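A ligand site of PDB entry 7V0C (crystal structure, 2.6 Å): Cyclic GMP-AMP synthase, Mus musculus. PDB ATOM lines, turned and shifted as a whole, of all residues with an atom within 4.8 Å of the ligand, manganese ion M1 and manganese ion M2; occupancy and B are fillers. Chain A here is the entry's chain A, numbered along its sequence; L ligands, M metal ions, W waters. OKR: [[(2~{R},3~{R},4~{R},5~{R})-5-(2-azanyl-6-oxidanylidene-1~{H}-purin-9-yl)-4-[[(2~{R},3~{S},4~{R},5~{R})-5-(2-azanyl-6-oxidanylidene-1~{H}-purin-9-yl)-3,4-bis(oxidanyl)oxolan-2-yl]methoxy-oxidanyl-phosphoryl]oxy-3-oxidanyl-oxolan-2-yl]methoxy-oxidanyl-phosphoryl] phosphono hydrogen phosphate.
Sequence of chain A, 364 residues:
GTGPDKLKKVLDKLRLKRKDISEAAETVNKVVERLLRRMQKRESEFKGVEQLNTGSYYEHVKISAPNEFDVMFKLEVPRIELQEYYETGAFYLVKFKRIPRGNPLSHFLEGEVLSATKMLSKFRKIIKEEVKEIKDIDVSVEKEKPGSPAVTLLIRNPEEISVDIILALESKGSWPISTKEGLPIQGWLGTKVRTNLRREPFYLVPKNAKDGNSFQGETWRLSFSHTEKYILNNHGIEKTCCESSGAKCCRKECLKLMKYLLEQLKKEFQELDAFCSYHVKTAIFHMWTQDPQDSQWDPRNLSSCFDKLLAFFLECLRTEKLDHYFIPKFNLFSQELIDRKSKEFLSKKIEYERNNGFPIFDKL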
ATOM      1  N   GLY A  55     -11.849  18.945  22.058  1.00  0.00           N
ATOM      2  CA  GLY A  55     -13.143  18.297  21.889  1.00  0.00           C
ATOM      3  C   GLY A  55     -13.228  16.930  22.491  1.00  0.00           C
ATOM      4  O   GLY A  55     -12.311  16.475  23.184  1.00  0.00           O
ATOM      5  N   SER A  56     -14.345  16.252  22.206  1.00  0.00           N
ATOM      6  CA  SER A  56     -14.774  15.078  22.956  1.00  0.00           C
ATOM      7  C   SER A  56     -13.787  13.931  22.893  1.00  0.00           C
ATOM      8  O   SER A  56     -13.537  13.269  23.887  1.00  0.00           O
ATOM      9  CB  SER A  56     -16.186  14.641  22.515  1.00  0.00           C
ATOM     10  OG  SER A  56     -16.247  14.403  21.130  1.00  0.00           O
ATOM     11  N   GLU A  59     -10.948  14.574  25.140  1.00  0.00           N
ATOM     12  CA  GLU A  59     -11.451  14.636  26.506  1.00  0.00           C
ATOM     13  C   GLU A  59     -11.927  13.244  26.997  1.00  0.00           C
ATOM     14  O   GLU A  59     -12.252  13.075  28.168  1.00  0.00           O
ATOM     15  CB  GLU A  59     -12.583  15.648  26.592  1.00  0.00           C
ATOM     16  CG  GLU A  59     -12.177  17.096  26.305  1.00  0.00           C
ATOM     17  CD  GLU A  59     -13.368  18.023  26.059  1.00  0.00           C
ATOM     18  OE1 GLU A  59     -14.484  17.534  25.760  1.00  0.00           O
ATOM     19  OE2 GLU A  59     -13.199  19.269  26.151  1.00  0.00           O
ATOM     20  N   LYS A  62     -16.082  11.097  23.824  1.00  0.00           N
ATOM     21  CA  LYS A  62     -16.633  10.808  22.517  1.00  0.00           C
ATOM     22  C   LYS A  62     -17.398   9.514  22.642  1.00  0.00           C
ATOM     23  O   LYS A  62     -16.879   8.547  23.171  1.00  0.00           O
ATOM     24  CB  LYS A  62     -15.526  10.651  21.464  1.00  0.00           C
ATOM     25  CG  LYS A  62     -16.043  10.425  20.045  1.00  0.00           C
ATOM     26  CD  LYS A  62     -16.568  11.711  19.416  1.00  0.00           C
ATOM     27  CE  LYS A  62     -17.110  11.428  18.015  1.00  0.00           C
ATOM     28  NZ  LYS A  62     -18.368  10.646  18.017  1.00  0.00           N
ATOM     29  N   GLU A  68     -15.550  11.854  14.684  1.00  0.00           N
ATOM     30  CA  GLU A  68     -15.518  13.301  14.664  1.00  0.00           C
ATOM     31  C   GLU A  68     -14.405  13.780  15.602  1.00  0.00           C
ATOM     32  O   GLU A  68     -14.415  13.482  16.786  1.00  0.00           O
ATOM     33  CB  GLU A  68     -16.900  13.878  15.030  1.00  0.00           C
ATOM     34  CG  GLU A  68     -17.187  15.284  14.507  1.00  0.00           C
ATOM     35  CD  GLU A  68     -16.634  16.386  15.425  1.00  0.00           C
ATOM     36  OE1 GLU A  68     -15.922  16.039  16.384  1.00  0.00           O
ATOM     37  OE2 GLU A  68     -16.897  17.603  15.195  1.00  0.00           O
ATOM     38  N   ASP A  70     -11.652  17.162  16.591  1.00  0.00           N
ATOM     39  CA  ASP A  70     -11.506  18.621  16.553  1.00  0.00           C
ATOM     40  C   ASP A  70     -10.056  19.003  16.834  1.00  0.00           C
ATOM     41  O   ASP A  70      -9.475  18.546  17.815  1.00  0.00           O
ATOM     42  CB  ASP A  70     -12.461  19.291  17.543  1.00  0.00           C
ATOM     43  CG  ASP A  70     -13.881  18.772  17.397  1.00  0.00           C
ATOM     44  OD1 ASP A  70     -14.546  19.103  16.383  1.00  0.00           O
ATOM     45  OD2 ASP A  70     -14.331  18.027  18.305  1.00  0.00           O
ATOM     46  N   LYS A 145     -20.177  25.748   5.843  1.00  0.00           N
ATOM     47  CA  LYS A 145     -21.372  26.096   6.568  1.00  0.00           C
ATOM     48  C   LYS A 145     -21.177  27.488   7.145  1.00  0.00           C
ATOM     49  O   LYS A 145     -20.172  27.742   7.792  1.00  0.00           O
ATOM     50  CB  LYS A 145     -21.624  25.117   7.706  1.00  0.00           C
ATOM     51  CG  LYS A 145     -21.932  23.719   7.211  1.00  0.00           C
ATOM     52  CD  LYS A 145     -22.606  22.905   8.313  1.00  0.00           C
ATOM     53  CE  LYS A 145     -22.511  21.405   8.067  1.00  0.00           C
ATOM     54  NZ  LYS A 145     -22.669  21.013   6.636  1.00  0.00           N
ATOM     55  N   GLY A 147     -21.592  30.534   9.841  1.00  0.00           N
ATOM     56  CA  GLY A 147     -21.558  30.491  11.285  1.00  0.00           C
ATOM     57  C   GLY A 147     -20.677  29.396  11.827  1.00  0.00           C
ATOM     58  O   GLY A 147     -20.842  29.019  12.979  1.00  0.00           O
ATOM     59  N   ASP A 164     -12.772  18.719  12.086  1.00  0.00           N
ATOM     60  CA  ASP A 164     -12.866  20.169  12.079  1.00  0.00           C
ATOM     61  C   ASP A 164     -11.492  20.750  12.382  1.00  0.00           C
ATOM     62  O   ASP A 164     -10.947  20.540  13.464  1.00  0.00           O
ATOM     63  CB  ASP A 164     -13.877  20.643  13.131  1.00  0.00           C
ATOM     64  CG  ASP A 164     -15.300  20.233  12.815  1.00  0.00           C
ATOM     65  OD1 ASP A 164     -15.661  20.012  11.627  1.00  0.00           O
ATOM     66  OD2 ASP A 164     -16.090  20.149  13.773  1.00  0.00           O
ATOM     67  N   ARG A 221     -14.844  35.165  17.964  1.00  0.00           N
ATOM     68  CA  ARG A 221     -15.488  34.608  19.194  1.00  0.00           C
ATOM     69  C   ARG A 221     -14.413  33.967  20.074  1.00  0.00           C
ATOM     70  O   ARG A 221     -13.502  33.311  19.517  1.00  0.00           O
ATOM     71  CB  ARG A 221     -16.570  33.578  18.822  1.00  0.00           C
ATOM     72  CG  ARG A 221     -17.588  33.295  19.927  1.00  0.00           C
ATOM     73  CD  ARG A 221     -18.156  31.889  19.836  1.00  0.00           C
ATOM     74  NE  ARG A 221     -17.158  30.905  20.223  1.00  0.00           N
ATOM     75  CZ  ARG A 221     -17.037  29.654  19.734  1.00  0.00           C
ATOM     76  NH1 ARG A 221     -17.858  29.200  18.794  1.00  0.00           N
ATOM     77  NH2 ARG A 221     -16.063  28.873  20.181  1.00  0.00           N
ATOM     78  N   LYS A 259     -25.128  13.622  26.451  1.00  0.00           N
ATOM     79  CA  LYS A 259     -24.709  13.792  25.056  1.00  0.00           C
ATOM     80  C   LYS A 259     -25.453  12.863  24.092  1.00  0.00           C
ATOM     81  O   LYS A 259     -25.877  13.289  23.007  1.00  0.00           O
ATOM     82  CB  LYS A 259     -23.229  13.508  24.919  1.00  0.00           C
ATOM     83  CG  LYS A 259     -22.329  14.643  25.351  1.00  0.00           C
ATOM     84  CD  LYS A 259     -20.884  14.174  25.423  1.00  0.00           C
ATOM     85  CE  LYS A 259     -20.254  13.886  24.070  1.00  0.00           C
ATOM     86  NZ  LYS A 259     -19.877  15.106  23.311  1.00  0.00           N
ATOM     87  N   GLU A 263     -27.937  13.716  20.932  1.00  0.00           N
ATOM     88  CA  GLU A 263     -27.643  13.165  19.600  1.00  0.00           C
ATOM     89  C   GLU A 263     -28.806  12.342  19.023  1.00  0.00           C
ATOM     90  O   GLU A 263     -29.195  12.531  17.870  1.00  0.00           O
ATOM     91  CB  GLU A 263     -26.382  12.280  19.606  1.00  0.00           C
ATOM     92  CG  GLU A 263     -25.066  13.029  19.598  1.00  0.00           C
ATOM     93  CD  GLU A 263     -23.855  12.122  19.453  1.00  0.00           C
ATOM     94  OE1 GLU A 263     -23.978  11.046  18.806  1.00  0.00           O
ATOM     95  OE2 GLU A 263     -22.763  12.509  19.973  1.00  0.00           O
ATOM     96  N   LYS A 266     -31.660  14.577  18.234  1.00  0.00           N
ATOM     97  CA  LYS A 266     -31.295  15.469  17.158  1.00  0.00           C
ATOM     98  C   LYS A 266     -31.340  14.800  15.789  1.00  0.00           C
ATOM     99  O   LYS A 266     -31.722  15.428  14.798  1.00  0.00           O
ATOM    100  CB  LYS A 266     -29.907  16.102  17.412  1.00  0.00           C
ATOM    101  CG  LYS A 266     -29.987  17.430  18.166  1.00  0.00           C
ATOM    102  CD  LYS A 266     -28.624  18.023  18.494  1.00  0.00           C
ATOM    103  CE  LYS A 266     -27.854  18.495  17.250  1.00  0.00           C
ATOM    104  NZ  LYS A 266     -28.578  19.542  16.504  1.00  0.00           N
ATOM    105  N   PHE A 275     -29.946  23.264  18.883  1.00  0.00           N
ATOM    106  CA  PHE A 275     -29.254  22.664  20.014  1.00  0.00           C
ATOM    107  C   PHE A 275     -27.999  21.905  19.601  1.00  0.00           C
ATOM    108  O   PHE A 275     -27.880  21.453  18.469  1.00  0.00           O
ATOM    109  CB  PHE A 275     -30.194  21.742  20.778  1.00  0.00           C
ATOM    110  CG  PHE A 275     -31.383  22.453  21.334  1.00  0.00           C
ATOM    111  CD1 PHE A 275     -31.269  23.248  22.464  1.00  0.00           C
ATOM    112  CD2 PHE A 275     -32.618  22.336  20.718  1.00  0.00           C
ATOM    113  CE1 PHE A 275     -32.362  23.919  22.971  1.00  0.00           C
ATOM    114  CE2 PHE A 275     -33.725  23.011  21.229  1.00  0.00           C
ATOM    115  CZ  PHE A 275     -33.590  23.795  22.358  1.00  0.00           C
ATOM    116  N   CYS A 276     -27.057  21.768  20.542  1.00  0.00           N
ATOM    117  CA  CYS A 276     -25.753  21.168  20.281  1.00  0.00           C
ATOM    118  C   CYS A 276     -25.159  20.595  21.557  1.00  0.00           C
ATOM    119  O   CYS A 276     -25.629  20.878  22.657  1.00  0.00           O
ATOM    120  CB  CYS A 276     -24.804  22.219  19.688  1.00  0.00           C
ATOM    121  SG  CYS A 276     -24.362  23.561  20.812  1.00  0.00           S
ATOM    122  N   SER A 277     -24.103  19.787  21.420  1.00  0.00           N
ATOM    123  CA  SER A 277     -23.494  19.142  22.550  1.00  0.00           C
ATOM    124  C   SER A 277     -22.872  20.155  23.516  1.00  0.00           C
ATOM    125  O   SER A 277     -22.739  19.877  24.715  1.00  0.00           O
ATOM    126  CB  SER A 277     -22.437  18.117  22.112  1.00  0.00           C
ATOM    127  OG  SER A 277     -21.403  18.732  21.374  1.00  0.00           O
ATOM    128  N   TYR A 278     -22.481  21.326  22.999  1.00  0.00           N
ATOM    129  CA  TYR A 278     -21.842  22.379  23.824  1.00  0.00           C
ATOM    130  C   TYR A 278     -22.818  22.866  24.903  1.00  0.00           C
ATOM    131  O   TYR A 278     -22.359  23.302  25.975  1.00  0.00           O
ATOM    132  CB  TYR A 278     -21.307  23.554  22.999  1.00  0.00           C
ATOM    133  CG  TYR A 278     -20.383  24.408  23.825  1.00  0.00           C
ATOM    134  CD1 TYR A 278     -19.126  23.922  24.157  1.00  0.00           C
ATOM    135  CD2 TYR A 278     -20.771  25.626  24.351  1.00  0.00           C
ATOM    136  CE1 TYR A 278     -18.259  24.650  24.963  1.00  0.00           C
ATOM    137  CE2 TYR A 278     -19.917  26.368  25.152  1.00  0.00           C
ATOM    138  CZ  TYR A 278     -18.661  25.874  25.462  1.00  0.00           C
ATOM    139  OH  TYR A 278     -17.796  26.583  26.256  1.00  0.00           O
ATOM    140  N   LYS A 281     -22.530  20.301  27.603  1.00  0.00           N
ATOM    141  CA  LYS A 281     -21.217  20.425  28.239  1.00  0.00           C
ATOM    142  C   LYS A 281     -21.202  21.582  29.232  1.00  0.00           C
ATOM    143  O   LYS A 281     -20.692  21.460  30.346  1.00  0.00           O
ATOM    144  CB  LYS A 281     -20.145  20.625  27.156  1.00  0.00           C
ATOM    145  CG  LYS A 281     -18.725  20.344  27.596  1.00  0.00           C
ATOM    146  CD  LYS A 281     -17.739  20.861  26.544  1.00  0.00           C
ATOM    147  CE  LYS A 281     -16.374  20.220  26.729  1.00  0.00           C
ATOM    148  NZ  LYS A 281     -15.291  20.921  25.951  1.00  0.00           N
ATOM    149  N   HIS A 324     -22.967  30.834  29.553  1.00  0.00           N
ATOM    150  CA  HIS A 324     -21.628  30.348  29.209  1.00  0.00           C
ATOM    151  C   HIS A 324     -20.829  30.276  30.499  1.00  0.00           C
ATOM    152  O   HIS A 324     -20.929  31.147  31.339  1.00  0.00           O
ATOM    153  CB  HIS A 324     -20.975  31.316  28.218  1.00  0.00           C
ATOM    154  CG  HIS A 324     -19.819  30.737  27.477  1.00  0.00           C
ATOM    155  ND1 HIS A 324     -18.627  30.403  28.086  1.00  0.00           N
ATOM    156  CD2 HIS A 324     -19.657  30.471  26.159  1.00  0.00           C
ATOM    157  CE1 HIS A 324     -17.788  29.944  27.175  1.00  0.00           C
ATOM    158  NE2 HIS A 324     -18.383  29.972  26.001  1.00  0.00           N
HETATM  159  N1  OKR L   1     -19.825  17.423  16.503  1.00  0.00           N
HETATM  160  C1  OKR L   1     -20.990  18.077  16.628  1.00  0.00           C
HETATM  161  N2  OKR L   1     -21.397  18.912  15.667  1.00  0.00           N
HETATM  162  C2  OKR L   1     -22.580  19.492  15.960  1.00  0.00           C
HETATM  163  C3  OKR L   1     -23.372  19.317  17.076  1.00  0.00           C
HETATM  164  N3  OKR L   1     -24.522  20.095  16.982  1.00  0.00           N
HETATM  165  C4  OKR L   1     -24.406  20.716  15.829  1.00  0.00           C
HETATM  166  N4  OKR L   1     -23.247  20.384  15.168  1.00  0.00           N
HETATM  167  C5  OKR L   1     -22.781  20.869  13.859  1.00  0.00           C
HETATM  168  O1  OKR L   1     -22.170  22.128  14.016  1.00  0.00           O
HETATM  169  C6  OKR L   1     -22.368  22.923  12.815  1.00  0.00           C
HETATM  170  C7  OKR L   1     -23.082  24.207  13.161  1.00  0.00           C
HETATM  171  O2  OKR L   1     -22.384  24.885  14.242  1.00  0.00           O
HETATM  172  P1  OKR L   1     -23.025  24.967  15.711  1.00  0.00           P
HETATM  173  O3  OKR L   1     -22.621  26.272  16.339  1.00  0.00           O
HETATM  174  O4  OKR L   1     -24.492  24.652  15.693  1.00  0.00           O
HETATM  175  O5  OKR L   1     -22.250  23.728  16.400  1.00  0.00           O
HETATM  176  C8  OKR L   1     -21.239  24.075  17.332  1.00  0.00           C
HETATM  177  C9  OKR L   1     -20.259  22.914  17.467  1.00  0.00           C
HETATM  178  O6  OKR L   1     -20.040  22.230  16.228  1.00  0.00           O
HETATM  179  C10 OKR L   1     -20.992  22.013  18.462  1.00  0.00           C
HETATM  180  C11 OKR L   1     -20.131  21.064  19.262  1.00  0.00           C
HETATM  181  O7  OKR L   1     -19.204  20.399  18.368  1.00  0.00           O
HETATM  182  P2  OKR L   1     -17.757  19.955  18.909  1.00  0.00           P
HETATM  183  O8  OKR L   1     -16.955  21.185  19.178  1.00  0.00           O
HETATM  184  O9  OKR L   1     -17.194  18.901  18.014  1.00  0.00           O
HETATM  185  O10 OKR L   1     -18.134  19.240  20.283  1.00  0.00           O
HETATM  186  P3  OKR L   1     -17.363  18.263  21.296  1.00  0.00           P
HETATM  187  O11 OKR L   1     -17.290  18.945  22.625  1.00  0.00           O
HETATM  188  O12 OKR L   1     -16.111  17.761  20.663  1.00  0.00           O
HETATM  189  O13 OKR L   1     -18.424  17.069  21.352  1.00  0.00           O
HETATM  190  P4  OKR L   1     -19.014  16.117  20.180  1.00  0.00           P
HETATM  191  O14 OKR L   1     -18.249  16.488  18.935  1.00  0.00           O
HETATM  192  O15 OKR L   1     -20.477  16.449  20.074  1.00  0.00           O
HETATM  193  O16 OKR L   1     -18.767  14.686  20.605  1.00  0.00           O
HETATM  194  O17 OKR L   1     -21.641  22.940  19.367  1.00  0.00           O
HETATM  195  C12 OKR L   1     -21.831  24.192  18.732  1.00  0.00           C
HETATM  196  N5  OKR L   1     -21.226  25.230  19.561  1.00  0.00           N
HETATM  197  C13 OKR L   1     -21.813  26.426  19.922  1.00  0.00           C
HETATM  198  N6  OKR L   1     -21.046  27.172  20.670  1.00  0.00           N
HETATM  199  C14 OKR L   1     -19.881  26.427  20.827  1.00  0.00           C
HETATM  200  C15 OKR L   1     -18.690  26.714  21.540  1.00  0.00           C
HETATM  201  O18 OKR L   1     -18.432  27.735  22.198  1.00  0.00           O
HETATM  202  N7  OKR L   1     -17.757  25.682  21.428  1.00  0.00           N
HETATM  203  C16 OKR L   1     -17.954  24.510  20.731  1.00  0.00           C
HETATM  204  N8  OKR L   1     -16.947  23.622  20.742  1.00  0.00           N
HETATM  205  N9  OKR L   1     -19.076  24.229  20.059  1.00  0.00           N
HETATM  206  C17 OKR L   1     -19.982  25.222  20.145  1.00  0.00           C
HETATM  207  C18 OKR L   1     -23.116  21.988  11.844  1.00  0.00           C
HETATM  208  O19 OKR L   1     -22.219  21.245  11.043  1.00  0.00           O
HETATM  209  C19 OKR L   1     -23.868  21.077  12.815  1.00  0.00           C
HETATM  210  O20 OKR L   1     -24.293  19.880  12.196  1.00  0.00           O
HETATM  211  C20 OKR L   1     -22.940  18.441  18.099  1.00  0.00           C
HETATM  212  O21 OKR L   1     -23.507  18.146  19.158  1.00  0.00           O
HETATM  213  N10 OKR L   1     -21.709  17.852  17.773  1.00  0.00           N
HETATM  214 MN    MN M   1     -16.585  19.585  15.750  1.00  0.00          MN
HETATM  215 MN    MN M   2     -16.276  17.000  18.414  1.00  0.00          MN
HETATM  216  O   HOH W   1     -15.133  15.256  18.897  1.00  0.00           O
HETATM  217  O   HOH W   2     -19.738  19.986  23.410  1.00  0.00           O
HETATM  218  O   HOH W   3     -19.678  12.286  20.498  1.00  0.00           O
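Water W1 bridges the side-chain hydroxyl of Ser 56 (2.6 Å) and the backbone carbonyl oxygen of Glu 68 (2.8 Å).
Water W3 lies within hydrogen-bond range of O16 of the ligand (2.6 Å), OE2 of Glu 263 (3.1 Å) and NZ of Lys 62 (3.2 Å).
Water W2 lies within hydrogen-bond range of O11 of the ligand, OG of Ser 277 and N of Tyr 278.
The side-chain carboxylate (OE2) of Glu 68 binds manganese ion M1 (2.1 Å).
OD2 of Asp 164 is bound to manganese ion M1, 2.1 Å away.
The side-chain carboxylate (OD1) of Asp 70 is bound to manganese ion M1 (2.2 Å).
O9 of the ligand binds manganese ion M1 (2.4 Å).
Three residues have an atom within 4 Å of manganese ion M1: Glu 68, Asp 70 and Asp 164.
Ser 56 touches manganese ion M2.
Within 4 Å of manganese ion M2: Ser 56, Glu 68 and Asp 70.
The nearest printed residue that does not touch manganese ion M2 is Gly 55 (4.9 Å).
Manganese ion M2 is bound by O14 of the ligand (2.1 Å), water W1 (2.1 Å), O9 of the ligand (2.1 Å), OD2 of Asp 70 (2.2 Å), OE1 of Glu 68 (2.3 Å) and O12 of the ligand (2.4 Å).
Manganese ion M2 has six donor atoms within binding distance.
The backbone carbonyl oxygen of Ser 56 sits at hydrogen-bond distance from the backbone NH of Lys 62 (3.3 Å).
The side-chain amino group (NZ) of Lys 266 is in hydrogen-bond range of the backbone carbonyl oxygen (O) of Phe 275 (2.8 Å).
N of Tyr 278 lies close to SG of Cys 276, at 3.6 Å.
A ring nitrogen (NE2) of His 324 is in hydrogen-bond range of the side-chain hydroxyl (OH) of Tyr 278 (3.4 Å).
Gly 55 touches the ligand (CA to O12, 3.3 Å).
Lys 62 touches the ligand (CD to O16, 3.9 Å).
Lys 145 touches the ligand.
Lys 266 touches the ligand (CE to N3, 3.7 Å).
Phe 275 touches the ligand.
Tyr 278 touches the ligand (CD1 to N7, 3.5 Å).
Hydrophobic or aromatic side chains within 4 Å of the ligand: Tyr 278.
Of the 19 residues printed, 13 come within 4 Å of the ligand.
The nearest printed residue that does not touch the ligand is Lys 281 (4.4 Å).
O16 of the ligand sits at hydrogen-bond distance from OG of Ser 56 (2.6 Å).
An oxygen (O17) of the ligand lies within hydrogen-bond range of the side-chain sulfur of Cys 276, 3.1 Å away.
The guanidinium group (NH2) of Arg 221 is in hydrogen-bond range of an oxygen (O18) of the ligand (3.3 Å).
An oxygen (O12) of the ligand lies close to the backbone NH of Ser 56 (2.8 Å).
An oxygen (O15) of the ligand lies within hydrogen-bond range of the side-chain hydroxyl (OG) of Ser 277 (2.8 Å).
The side-chain amino group (NZ) of Lys 259 is in salt-bridge range of an oxygen (O16) of the ligand, 3.0 Å away.
An oxygen (O21) of the ligand sits at hydrogen-bond distance from the backbone NH (N) of Ser 277 (2.9 Å).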
